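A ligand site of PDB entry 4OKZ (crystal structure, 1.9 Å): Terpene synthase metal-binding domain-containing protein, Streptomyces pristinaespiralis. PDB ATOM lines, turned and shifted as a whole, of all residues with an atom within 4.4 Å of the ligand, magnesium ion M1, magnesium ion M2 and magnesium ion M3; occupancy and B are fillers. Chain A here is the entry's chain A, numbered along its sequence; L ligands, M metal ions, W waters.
The guanidinium group (NE) of Arg 310 is in salt-bridge range of an oxygen (O6) of the ligand, at 2.8 Å. NZ of Lys 231 sits close to O7 of the ligand (2.6 Å). O1 of the ligand lies within hydrogen-bond range of NH2 of Arg 178 (3.0 Å). An oxygen (O6) of the ligand lies within hydrogen-bond range of the side-chain hydroxyl (OH) of Tyr 311 (2.8 Å).
The guanidinium group (NH2) of Arg 178 is in salt-bridge range of the side-chain carboxylate (OD2) of Asp 181 (2.9 Å). NH1 of Arg 310 is in salt-bridge range of OD2 of Asp 83. The side-chain amide nitrogen of Asn 224 sits at hydrogen-bond distance from the side-chain hydroxyl of Tyr 311, 3.3 Å away. The guanidinium group (NH1) of Arg 178 lies within hydrogen-bond range of the backbone carbonyl oxygen (O) of Thr 221 (3.5 Å). The side-chain carboxylate (OD1) of Asp 82 is in hydrogen-bond range of the side-chain hydroxyl (OH) of Tyr 152. The side-chain amide oxygen (OD1) of Asn 224 lies close to the guanidinium group (NH1) of Arg 178 (2.8 Å).
Residues that only touch the ligand: Phe 55 (3.8 Å), Leu 78 (3.4 Å), Phe 79 (3.4 Å), Tyr 152 (3.8 Å), Asp 181 (3.98 Å), Gly 182 (3.4 Å), Ala 183 (3.5 Å), Val 187 (3.8 Å) and Ile 220 (3.9 Å). Within 4 Å of the ligand: Phe 55, Leu 78, Phe 79, Asp 82, Glu 87, Tyr 152, Arg 178, Asp 181, Gly 182, Ala 183, Val 187, Ile 220, Asn 224, Ser 228, Lys 231, Glu 232, Arg 310 and Tyr 311. Along chain A the residues within 4 Å of the ligand span positions 55 to 311.
Two residues have an atom within 4 Å of magnesium ion M1: Asp 82 and Glu 87.
The nearest printed residue that does not touch magnesium ion M2 is Glu 159 (4.4 Å).
Arg 178 touches magnesium ion M3 (NH1 to MG, 3.9 Å). Within 4 Å of magnesium ion M3: Arg 178, Asn 224, Ser 228 and Glu 232. Along chain A the residues within 4 Å of magnesium ion M3 span positions 178 to 232. The nearest printed residue that does not touch magnesium ion M3 is Lys 231 (5.0 Å).
Magnesium ion M1 is bound by OE2 of Glu 87 (1.9 Å), O7 of the ligand (2.0 Å), O3 of the ligand (2.1 Å), water W4 (2.1 Å), water W8 (2.2 Å) and water W2 (2.4 Å). Magnesium ion M1 has six donor atoms within binding distance.
Magnesium ion M2 is bound by water W6 (2.1 Å), an oxygen (O3) of the ligand (2.1 Å), water W9 (2.1 Å), the side-chain carboxylate (OD2) of Asp 82 (2.1 Å), water W7 (2.2 Å) and the side-chain carboxylate (OE2) of Glu 87 (2.4 Å).
Water W5 binds magnesium ion M3, 2.0 Å away. O2 of the ligand binds magnesium ion M3 (2.1 Å). O5 of the ligand is bound to magnesium ion M3 (2.1 Å). Magnesium ion M3 is bound by OG of Ser 228. The side-chain amide oxygen (OD1) of Asn 224 binds magnesium ion M3 (2.2 Å). OE1 of Glu 232 is bound to magnesium ion M3 (2.2 Å). Magnesium ion M3 has six donor atoms within binding distance.
Water W4 lies within hydrogen-bond range of OD2 of Asp 83 (2.7 Å), NH1 of Arg 310 (3.2 Å) and O4 of the ligand (3.4 Å). Water W2 lies within hydrogen-bond range of OD2 of Asp 83 (2.8 Å), NZ of Lys 231 (3.1 Å) and NH1 of Arg 310 (3.4 Å). Water W8 bridges the side-chain carboxylate (OE1) of Glu 87 (2.7 Å) and the side-chain amino group (NZ) of Lys 231 (3.4 Å). Water W9 lies within hydrogen-bond range of O of Asp 181, O1 of the ligand and NH2 of Arg 178. Water W6 bridges the side-chain carboxylate of Glu 159 (2.9 Å) and the side-chain carboxylate of Glu 87 (3.5 Å). Water W5 bridges the side-chain carboxylate of Glu 232 (2.8 Å) and the guanidinium group of Arg 178 (3.4 Å).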
ATOM      1  N   PHE A  55      20.488 -18.284 -16.522  1.00  0.00           N
ATOM      2  CA  PHE A  55      20.995 -17.161 -17.331  1.00  0.00           C
ATOM      3  C   PHE A  55      21.470 -16.014 -16.439  1.00  0.00           C
ATOM      4  O   PHE A  55      22.597 -15.525 -16.580  1.00  0.00           O
ATOM      5  CB  PHE A  55      19.880 -16.714 -18.292  1.00  0.00           C
ATOM      6  CG  PHE A  55      20.217 -15.516 -19.149  1.00  0.00           C
ATOM      7  CD1 PHE A  55      21.533 -15.220 -19.519  1.00  0.00           C
ATOM      8  CD2 PHE A  55      19.202 -14.701 -19.619  1.00  0.00           C
ATOM      9  CE1 PHE A  55      21.814 -14.108 -20.308  1.00  0.00           C
ATOM     10  CE2 PHE A  55      19.463 -13.610 -20.418  1.00  0.00           C
ATOM     11  CZ  PHE A  55      20.772 -13.307 -20.765  1.00  0.00           C
ATOM     12  N   ILE A  75      14.151 -10.577 -15.763  1.00  0.00           N
ATOM     13  CA  ILE A  75      14.261 -11.117 -17.118  1.00  0.00           C
ATOM     14  C   ILE A  75      12.985 -11.904 -17.483  1.00  0.00           C
ATOM     15  O   ILE A  75      12.467 -11.751 -18.588  1.00  0.00           O
ATOM     16  CB  ILE A  75      15.517 -12.004 -17.289  1.00  0.00           C
ATOM     17  CG1 ILE A  75      16.772 -11.122 -17.216  1.00  0.00           C
ATOM     18  CG2 ILE A  75      15.494 -12.729 -18.632  1.00  0.00           C
ATOM     19  CD1 ILE A  75      18.067 -11.886 -17.055  1.00  0.00           C
ATOM     20  N   LEU A  78      10.321  -9.419 -18.184  1.00  0.00           N
ATOM     21  CA  LEU A  78      10.548  -8.798 -19.492  1.00  0.00           C
ATOM     22  C   LEU A  78      10.053  -9.696 -20.624  1.00  0.00           C
ATOM     23  O   LEU A  78       9.475  -9.206 -21.581  1.00  0.00           O
ATOM     24  CB  LEU A  78      12.019  -8.446 -19.687  1.00  0.00           C
ATOM     25  CG  LEU A  78      12.544  -7.240 -18.887  1.00  0.00           C
ATOM     26  CD1 LEU A  78      14.069  -7.223 -18.857  1.00  0.00           C
ATOM     27  CD2 LEU A  78      12.005  -5.943 -19.464  1.00  0.00           C
ATOM     28  N   PHE A  79      10.251 -11.009 -20.504  1.00  0.00           N
ATOM     29  CA  PHE A  79       9.678 -11.947 -21.482  1.00  0.00           C
ATOM     30  C   PHE A  79       8.153 -11.930 -21.407  1.00  0.00           C
ATOM     31  O   PHE A  79       7.489 -12.045 -22.434  1.00  0.00           O
ATOM     32  CB  PHE A  79      10.213 -13.364 -21.304  1.00  0.00           C
ATOM     33  CG  PHE A  79      11.573 -13.568 -21.889  1.00  0.00           C
ATOM     34  CD1 PHE A  79      12.660 -13.892 -21.081  1.00  0.00           C
ATOM     35  CD2 PHE A  79      11.789 -13.418 -23.248  1.00  0.00           C
ATOM     36  CE1 PHE A  79      13.913 -14.071 -21.622  1.00  0.00           C
ATOM     37  CE2 PHE A  79      13.042 -13.595 -23.803  1.00  0.00           C
ATOM     38  CZ  PHE A  79      14.108 -13.922 -22.987  1.00  0.00           C
ATOM     39  N   ASP A  82       7.555  -8.860 -23.476  1.00  0.00           N
ATOM     40  CA  ASP A  82       8.047  -8.961 -24.839  1.00  0.00           C
ATOM     41  C   ASP A  82       7.388 -10.095 -25.651  1.00  0.00           C
ATOM     42  O   ASP A  82       7.056  -9.897 -26.820  1.00  0.00           O
ATOM     43  CB  ASP A  82       9.551  -9.123 -24.843  1.00  0.00           C
ATOM     44  CG  ASP A  82      10.176  -8.591 -26.098  1.00  0.00           C
ATOM     45  OD1 ASP A  82      10.077  -7.380 -26.359  1.00  0.00           O
ATOM     46  OD2 ASP A  82      10.770  -9.405 -26.817  1.00  0.00           O
ATOM     47  N   ASP A  83       7.207 -11.263 -25.031  1.00  0.00           N
ATOM     48  CA  ASP A  83       6.441 -12.344 -25.653  1.00  0.00           C
ATOM     49  C   ASP A  83       4.944 -12.075 -25.547  1.00  0.00           C
ATOM     50  O   ASP A  83       4.222 -12.087 -26.549  1.00  0.00           O
ATOM     51  CB  ASP A  83       6.725 -13.706 -24.985  1.00  0.00           C
ATOM     52  CG  ASP A  83       8.125 -14.223 -25.241  1.00  0.00           C
ATOM     53  OD1 ASP A  83       8.499 -15.220 -24.584  1.00  0.00           O
ATOM     54  OD2 ASP A  83       8.843 -13.675 -26.096  1.00  0.00           O
ATOM     55  N   GLU A  87       5.327  -9.619 -29.082  1.00  0.00           N
ATOM     56  CA  GLU A  87       5.567 -10.554 -30.179  1.00  0.00           C
ATOM     57  C   GLU A  87       4.489 -11.618 -30.365  1.00  0.00           C
ATOM     58  O   GLU A  87       4.332 -12.135 -31.478  1.00  0.00           O
ATOM     59  CB  GLU A  87       6.925 -11.221 -30.020  1.00  0.00           C
ATOM     60  CG  GLU A  87       8.093 -10.253 -30.023  1.00  0.00           C
ATOM     61  CD  GLU A  87       9.402 -10.945 -30.310  1.00  0.00           C
ATOM     62  OE1 GLU A  87       9.617 -11.334 -31.473  1.00  0.00           O
ATOM     63  OE2 GLU A  87      10.217 -11.128 -29.377  1.00  0.00           O
ATOM     64  N   TYR A 152      13.731   0.814 -23.637  1.00  0.00           N
ATOM     65  CA  TYR A 152      13.218  -0.460 -24.132  1.00  0.00           C
ATOM     66  C   TYR A 152      11.776  -0.322 -24.650  1.00  0.00           C
ATOM     67  O   TYR A 152      11.481  -0.716 -25.782  1.00  0.00           O
ATOM     68  CB  TYR A 152      13.309  -1.539 -23.035  1.00  0.00           C
ATOM     69  CG  TYR A 152      12.447  -2.747 -23.286  1.00  0.00           C
ATOM     70  CD1 TYR A 152      12.617  -3.518 -24.428  1.00  0.00           C
ATOM     71  CD2 TYR A 152      11.437  -3.100 -22.398  1.00  0.00           C
ATOM     72  CE1 TYR A 152      11.809  -4.609 -24.684  1.00  0.00           C
ATOM     73  CE2 TYR A 152      10.630  -4.193 -22.641  1.00  0.00           C
ATOM     74  CZ  TYR A 152      10.819  -4.942 -23.787  1.00  0.00           C
ATOM     75  OH  TYR A 152       9.997  -6.037 -24.029  1.00  0.00           O
ATOM     76  N   GLU A 159       9.210  -1.101 -33.011  1.00  0.00           N
ATOM     77  CA  GLU A 159       9.133  -2.447 -33.597  1.00  0.00           C
ATOM     78  C   GLU A 159       7.681  -2.814 -33.949  1.00  0.00           C
ATOM     79  O   GLU A 159       7.420  -3.423 -34.986  1.00  0.00           O
ATOM     80  CB  GLU A 159       9.730  -3.494 -32.640  1.00  0.00           C
ATOM     81  CG  GLU A 159       9.800  -4.890 -33.223  1.00  0.00           C
ATOM     82  CD  GLU A 159      10.145  -5.959 -32.190  1.00  0.00           C
ATOM     83  OE1 GLU A 159       9.395  -6.084 -31.197  1.00  0.00           O
ATOM     84  OE2 GLU A 159      11.131  -6.681 -32.385  1.00  0.00           O
ATOM     85  N   ARG A 178      17.351  -2.122 -32.287  1.00  0.00           N
ATOM     86  CA  ARG A 178      17.787  -3.349 -31.625  1.00  0.00           C
ATOM     87  C   ARG A 178      18.719  -3.086 -30.434  1.00  0.00           C
ATOM     88  O   ARG A 178      18.755  -3.881 -29.492  1.00  0.00           O
ATOM     89  CB  ARG A 178      18.467  -4.258 -32.662  1.00  0.00           C
ATOM     90  CG  ARG A 178      18.786  -5.669 -32.182  1.00  0.00           C
ATOM     91  CD  ARG A 178      17.566  -6.381 -31.636  1.00  0.00           C
ATOM     92  NE  ARG A 178      17.824  -7.807 -31.414  1.00  0.00           N
ATOM     93  CZ  ARG A 178      17.183  -8.576 -30.538  1.00  0.00           C
ATOM     94  NH1 ARG A 178      17.513  -9.866 -30.427  1.00  0.00           N
ATOM     95  NH2 ARG A 178      16.227  -8.074 -29.763  1.00  0.00           N
ATOM     96  N   ASP A 181      15.670  -2.627 -28.007  1.00  0.00           N
ATOM     97  CA  ASP A 181      14.488  -3.495 -27.937  1.00  0.00           C
ATOM     98  C   ASP A 181      14.781  -4.899 -27.384  1.00  0.00           C
ATOM     99  O   ASP A 181      13.856  -5.649 -27.097  1.00  0.00           O
ATOM    100  CB  ASP A 181      13.669  -3.518 -29.245  1.00  0.00           C
ATOM    101  CG  ASP A 181      14.190  -4.489 -30.293  1.00  0.00           C
ATOM    102  OD1 ASP A 181      14.006  -4.183 -31.493  1.00  0.00           O
ATOM    103  OD2 ASP A 181      14.741  -5.555 -29.947  1.00  0.00           O
ATOM    104  N   GLY A 182      16.059  -5.210 -27.202  1.00  0.00           N
ATOM    105  CA  GLY A 182      16.466  -6.403 -26.448  1.00  0.00           C
ATOM    106  C   GLY A 182      16.536  -6.200 -24.930  1.00  0.00           C
ATOM    107  O   GLY A 182      16.905  -7.127 -24.205  1.00  0.00           O
ATOM    108  N   ALA A 183      16.210  -4.989 -24.467  1.00  0.00           N
ATOM    109  CA  ALA A 183      16.239  -4.653 -23.041  1.00  0.00           C
ATOM    110  C   ALA A 183      17.600  -4.811 -22.367  1.00  0.00           C
ATOM    111  O   ALA A 183      17.697  -4.914 -21.147  1.00  0.00           O
ATOM    112  CB  ALA A 183      15.163  -5.437 -22.289  1.00  0.00           C
ATOM    113  N   THR A 184      18.670  -4.814 -23.154  1.00  0.00           N
ATOM    114  CA  THR A 184      20.009  -4.994 -22.618  1.00  0.00           C
ATOM    115  C   THR A 184      20.391  -3.828 -21.699  1.00  0.00           C
ATOM    116  O   THR A 184      21.129  -4.013 -20.728  1.00  0.00           O
ATOM    117  CB  THR A 184      21.055  -5.129 -23.740  1.00  0.00           C
ATOM    118  OG1 THR A 184      20.891  -4.071 -24.674  1.00  0.00           O
ATOM    119  CG2 THR A 184      20.891  -6.472 -24.451  1.00  0.00           C
ATOM    120  N   VAL A 187      19.335  -4.093 -17.846  1.00  0.00           N
ATOM    121  CA  VAL A 187      20.130  -5.002 -17.018  1.00  0.00           C
ATOM    122  C   VAL A 187      21.311  -4.289 -16.367  1.00  0.00           C
ATOM    123  O   VAL A 187      21.709  -4.615 -15.249  1.00  0.00           O
ATOM    124  CB  VAL A 187      20.632  -6.199 -17.871  1.00  0.00           C
ATOM    125  CG1 VAL A 187      21.642  -7.050 -17.106  1.00  0.00           C
ATOM    126  CG2 VAL A 187      19.459  -7.045 -18.321  1.00  0.00           C
ATOM    127  N   ILE A 220      25.270  -8.889 -27.820  1.00  0.00           N
ATOM    128  CA  ILE A 220      24.237  -9.704 -27.174  1.00  0.00           C
ATOM    129  C   ILE A 220      23.012  -9.872 -28.090  1.00  0.00           C
ATOM    130  O   ILE A 220      22.506 -10.987 -28.232  1.00  0.00           O
ATOM    131  CB  ILE A 220      23.837  -9.097 -25.814  1.00  0.00           C
ATOM    132  CG1 ILE A 220      24.988  -9.283 -24.814  1.00  0.00           C
ATOM    133  CG2 ILE A 220      22.561  -9.744 -25.263  1.00  0.00           C
ATOM    134  CD1 ILE A 220      24.875  -8.410 -23.580  1.00  0.00           C
ATOM    135  N   THR A 221      22.568  -8.794 -28.710  1.00  0.00           N
ATOM    136  CA  THR A 221      21.392  -8.863 -29.584  1.00  0.00           C
ATOM    137  C   THR A 221      21.694  -9.563 -30.919  1.00  0.00           C
ATOM    138  O   THR A 221      20.835 -10.283 -31.432  1.00  0.00           O
ATOM    139  CB  THR A 221      20.753  -7.477 -29.814  1.00  0.00           C
ATOM    140  OG1 THR A 221      21.730  -6.542 -30.289  1.00  0.00           O
ATOM    141  CG2 THR A 221      20.132  -6.948 -28.530  1.00  0.00           C
ATOM    142  N   ASN A 224      21.928 -13.190 -30.143  1.00  0.00           N
ATOM    143  CA  ASN A 224      20.559 -13.673 -30.036  1.00  0.00           C
ATOM    144  C   ASN A 224      19.896 -13.796 -31.400  1.00  0.00           C
ATOM    145  O   ASN A 224      19.250 -14.800 -31.677  1.00  0.00           O
ATOM    146  CB  ASN A 224      19.723 -12.789 -29.112  1.00  0.00           C
ATOM    147  CG  ASN A 224      18.266 -13.191 -29.112  1.00  0.00           C
ATOM    148  OD1 ASN A 224      17.480 -12.629 -29.858  1.00  0.00           O
ATOM    149  ND2 ASN A 224      17.904 -14.188 -28.316  1.00  0.00           N
ATOM    150  N   SER A 228      18.589 -17.337 -32.091  1.00  0.00           N
ATOM    151  CA  SER A 228      17.123 -17.370 -32.054  1.00  0.00           C
ATOM    152  C   SER A 228      16.475 -17.336 -33.438  1.00  0.00           C
ATOM    153  O   SER A 228      15.259 -17.426 -33.555  1.00  0.00           O
ATOM    154  CB  SER A 228      16.551 -16.249 -31.146  1.00  0.00           C
ATOM    155  OG  SER A 228      16.544 -14.956 -31.748  1.00  0.00           O
ATOM    156  N   LYS A 231      14.101 -20.491 -34.033  1.00  0.00           N
ATOM    157  CA  LYS A 231      12.785 -20.457 -33.376  1.00  0.00           C
ATOM    158  C   LYS A 231      11.918 -19.308 -33.892  1.00  0.00           C
ATOM    159  O   LYS A 231      10.699 -19.426 -33.963  1.00  0.00           O
ATOM    160  CB  LYS A 231      12.920 -20.434 -31.838  1.00  0.00           C
ATOM    161  CG  LYS A 231      13.325 -19.097 -31.222  1.00  0.00           C
ATOM    162  CD  LYS A 231      12.114 -18.267 -30.795  1.00  0.00           C
ATOM    163  CE  LYS A 231      12.537 -17.035 -30.018  1.00  0.00           C
ATOM    164  NZ  LYS A 231      11.379 -16.169 -29.659  1.00  0.00           N
ATOM    165  N   GLU A 232      12.556 -18.202 -34.272  1.00  0.00           N
ATOM    166  CA  GLU A 232      11.830 -17.023 -34.775  1.00  0.00           C
ATOM    167  C   GLU A 232      11.258 -17.226 -36.169  1.00  0.00           C
ATOM    168  O   GLU A 232      10.074 -16.961 -36.396  1.00  0.00           O
ATOM    169  CB  GLU A 232      12.720 -15.789 -34.742  1.00  0.00           C
ATOM    170  CG  GLU A 232      12.898 -15.286 -33.331  1.00  0.00           C
ATOM    171  CD  GLU A 232      13.860 -14.113 -33.189  1.00  0.00           C
ATOM    172  OE1 GLU A 232      13.920 -13.616 -32.062  1.00  0.00           O
ATOM    173  OE2 GLU A 232      14.537 -13.703 -34.157  1.00  0.00           O
ATOM    174  N   PHE A 297      27.966 -10.616 -18.884  1.00  0.00           N
ATOM    175  CA  PHE A 297      26.664 -10.487 -19.537  1.00  0.00           C
ATOM    176  C   PHE A 297      26.746 -11.037 -20.963  1.00  0.00           C
ATOM    177  O   PHE A 297      25.917 -11.831 -21.381  1.00  0.00           O
ATOM    178  CB  PHE A 297      26.250  -9.002 -19.501  1.00  0.00           C
ATOM    179  CG  PHE A 297      24.832  -8.710 -19.960  1.00  0.00           C
ATOM    180  CD1 PHE A 297      23.863  -9.711 -20.097  1.00  0.00           C
ATOM    181  CD2 PHE A 297      24.454  -7.393 -20.194  1.00  0.00           C
ATOM    182  CE1 PHE A 297      22.572  -9.396 -20.499  1.00  0.00           C
ATOM    183  CE2 PHE A 297      23.163  -7.078 -20.597  1.00  0.00           C
ATOM    184  CZ  PHE A 297      22.215  -8.077 -20.741  1.00  0.00           C
ATOM    185  N   TRP A 304      23.855 -19.349 -22.547  1.00  0.00           N
ATOM    186  CA  TRP A 304      22.413 -19.557 -22.417  1.00  0.00           C
ATOM    187  C   TRP A 304      21.751 -19.699 -23.784  1.00  0.00           C
ATOM    188  O   TRP A 304      20.867 -20.534 -23.970  1.00  0.00           O
ATOM    189  CB  TRP A 304      21.806 -18.389 -21.629  1.00  0.00           C
ATOM    190  CG  TRP A 304      20.354 -18.527 -21.366  1.00  0.00           C
ATOM    191  CD1 TRP A 304      19.739 -19.486 -20.621  1.00  0.00           C
ATOM    192  CD2 TRP A 304      19.334 -17.654 -21.827  1.00  0.00           C
ATOM    193  NE1 TRP A 304      18.387 -19.264 -20.598  1.00  0.00           N
ATOM    194  CE2 TRP A 304      18.108 -18.145 -21.332  1.00  0.00           C
ATOM    195  CE3 TRP A 304      19.327 -16.485 -22.612  1.00  0.00           C
ATOM    196  CZ2 TRP A 304      16.893 -17.520 -21.603  1.00  0.00           C
ATOM    197  CZ3 TRP A 304      18.120 -15.870 -22.878  1.00  0.00           C
ATOM    198  CH2 TRP A 304      16.918 -16.393 -22.368  1.00  0.00           C
ATOM    199  N   ARG A 310      14.321 -22.546 -25.059  1.00  0.00           N
ATOM    200  CA  ARG A 310      13.792 -21.415 -25.804  1.00  0.00           C
ATOM    201  C   ARG A 310      14.376 -21.358 -27.225  1.00  0.00           C
ATOM    202  O   ARG A 310      13.688 -20.999 -28.178  1.00  0.00           O
ATOM    203  CB  ARG A 310      14.096 -20.119 -25.041  1.00  0.00           C
ATOM    204  CG  ARG A 310      13.258 -18.947 -25.498  1.00  0.00           C
ATOM    205  CD  ARG A 310      13.599 -17.677 -24.747  1.00  0.00           C
ATOM    206  NE  ARG A 310      12.932 -16.569 -25.420  1.00  0.00           N
ATOM    207  CZ  ARG A 310      11.644 -16.242 -25.255  1.00  0.00           C
ATOM    208  NH1 ARG A 310      11.149 -15.237 -25.956  1.00  0.00           N
ATOM    209  NH2 ARG A 310      10.865 -16.896 -24.399  1.00  0.00           N
ATOM    210  N   TYR A 311      15.659 -21.710 -27.358  1.00  0.00           N
ATOM    211  CA  TYR A 311      16.363 -21.614 -28.641  1.00  0.00           C
ATOM    212  C   TYR A 311      16.648 -22.972 -29.290  1.00  0.00           C
ATOM    213  O   TYR A 311      16.619 -23.087 -30.510  1.00  0.00           O
ATOM    214  CB  TYR A 311      17.649 -20.820 -28.446  1.00  0.00           C
ATOM    215  CG  TYR A 311      17.403 -19.497 -27.754  1.00  0.00           C
ATOM    216  CD1 TYR A 311      17.918 -19.238 -26.485  1.00  0.00           C
ATOM    217  CD2 TYR A 311      16.599 -18.523 -28.350  1.00  0.00           C
ATOM    218  CE1 TYR A 311      17.667 -18.040 -25.840  1.00  0.00           C
ATOM    219  CE2 TYR A 311      16.348 -17.315 -27.703  1.00  0.00           C
ATOM    220  CZ  TYR A 311      16.879 -17.083 -26.454  1.00  0.00           C
ATOM    221  OH  TYR A 311      16.628 -15.882 -25.823  1.00  0.00           O
HETATM  222  C1  LIG L   1      15.271 -10.001 -26.400  1.00  0.00           C
HETATM  223  O1  LIG L   1      15.072 -10.080 -27.801  1.00  0.00           O
HETATM  224  C2  LIG L   1      13.998  -9.412 -25.823  1.00  0.00           C
HETATM  225  C3  LIG L   1      14.183  -9.129 -24.303  1.00  0.00           C
HETATM  226  C4  LIG L   1      13.170  -8.046 -23.894  1.00  0.00           C
HETATM  227  C5  LIG L   1      14.015 -10.391 -23.469  1.00  0.00           C
HETATM  228  C6  LIG L   1      14.537 -10.019 -22.083  1.00  0.00           C
HETATM  229  C7  LIG L   1      16.015 -10.447 -22.019  1.00  0.00           C
HETATM  230  C8  LIG L   1      17.082  -9.563 -21.352  1.00  0.00           C
HETATM  231  C9  LIG L   1      16.759  -8.249 -20.637  1.00  0.00           C
HETATM  232  C10 LIG L   1      18.504 -10.015 -21.362  1.00  0.00           C
HETATM  233  C11 LIG L   1      18.967  -9.784 -22.788  1.00  0.00           C
HETATM  234  C12 LIG L   1      19.033 -11.158 -23.439  1.00  0.00           C
HETATM  235  C13 LIG L   1      18.939 -11.333 -24.959  1.00  0.00           C
HETATM  236  C14 LIG L   1      19.053 -12.739 -25.517  1.00  0.00           C
HETATM  237  C15 LIG L   1      18.736 -10.160 -25.931  1.00  0.00           C
HETATM  238  P1  LIG L   1      14.209 -11.229 -28.559  1.00  0.00           P
HETATM  239  O2  LIG L   1      14.969 -11.571 -29.933  1.00  0.00           O
HETATM  240  O3  LIG L   1      12.948 -10.665 -28.917  1.00  0.00           O
HETATM  241  O4  LIG L   1      14.225 -12.450 -27.567  1.00  0.00           O
HETATM  242  P2  LIG L   1      13.779 -13.851 -28.056  1.00  0.00           P
HETATM  243  O5  LIG L   1      14.877 -14.176 -29.173  1.00  0.00           O
HETATM  244  O6  LIG L   1      14.334 -14.707 -26.982  1.00  0.00           O
HETATM  245  O7  LIG L   1      12.417 -14.045 -28.491  1.00  0.00           O
HETATM  246 MG    MG M   1      11.594 -12.254 -28.745  1.00  0.00          MG
HETATM  247 MG    MG M   2      11.534  -9.181 -28.812  1.00  0.00          MG
HETATM  248 MG    MG M   3      15.683 -13.277 -30.858  1.00  0.00          MG
HETATM  249  O   HOH W   1      13.642 -10.458 -32.330  1.00  0.00           O
HETATM  250  O   HOH W   2       9.692 -13.773 -28.717  1.00  0.00           O
HETATM  251  O   HOH W   3      19.635 -15.356 -26.528  1.00  0.00           O
HETATM  252  O   HOH W   4      10.928 -12.125 -26.742  1.00  0.00           O
HETATM  253  O   HOH W   5      16.264 -12.223 -32.482  1.00  0.00           O
HETATM  254  O   HOH W   6      12.009  -8.893 -30.788  1.00  0.00           O
HETATM  255  O   HOH W   7      10.064  -7.649 -29.170  1.00  0.00           O
HETATM  256  O   HOH W   8      11.662 -12.971 -30.799  1.00  0.00           O
HETATM  257  O   HOH W   9      13.007  -7.791 -28.438  1.00  0.00           O
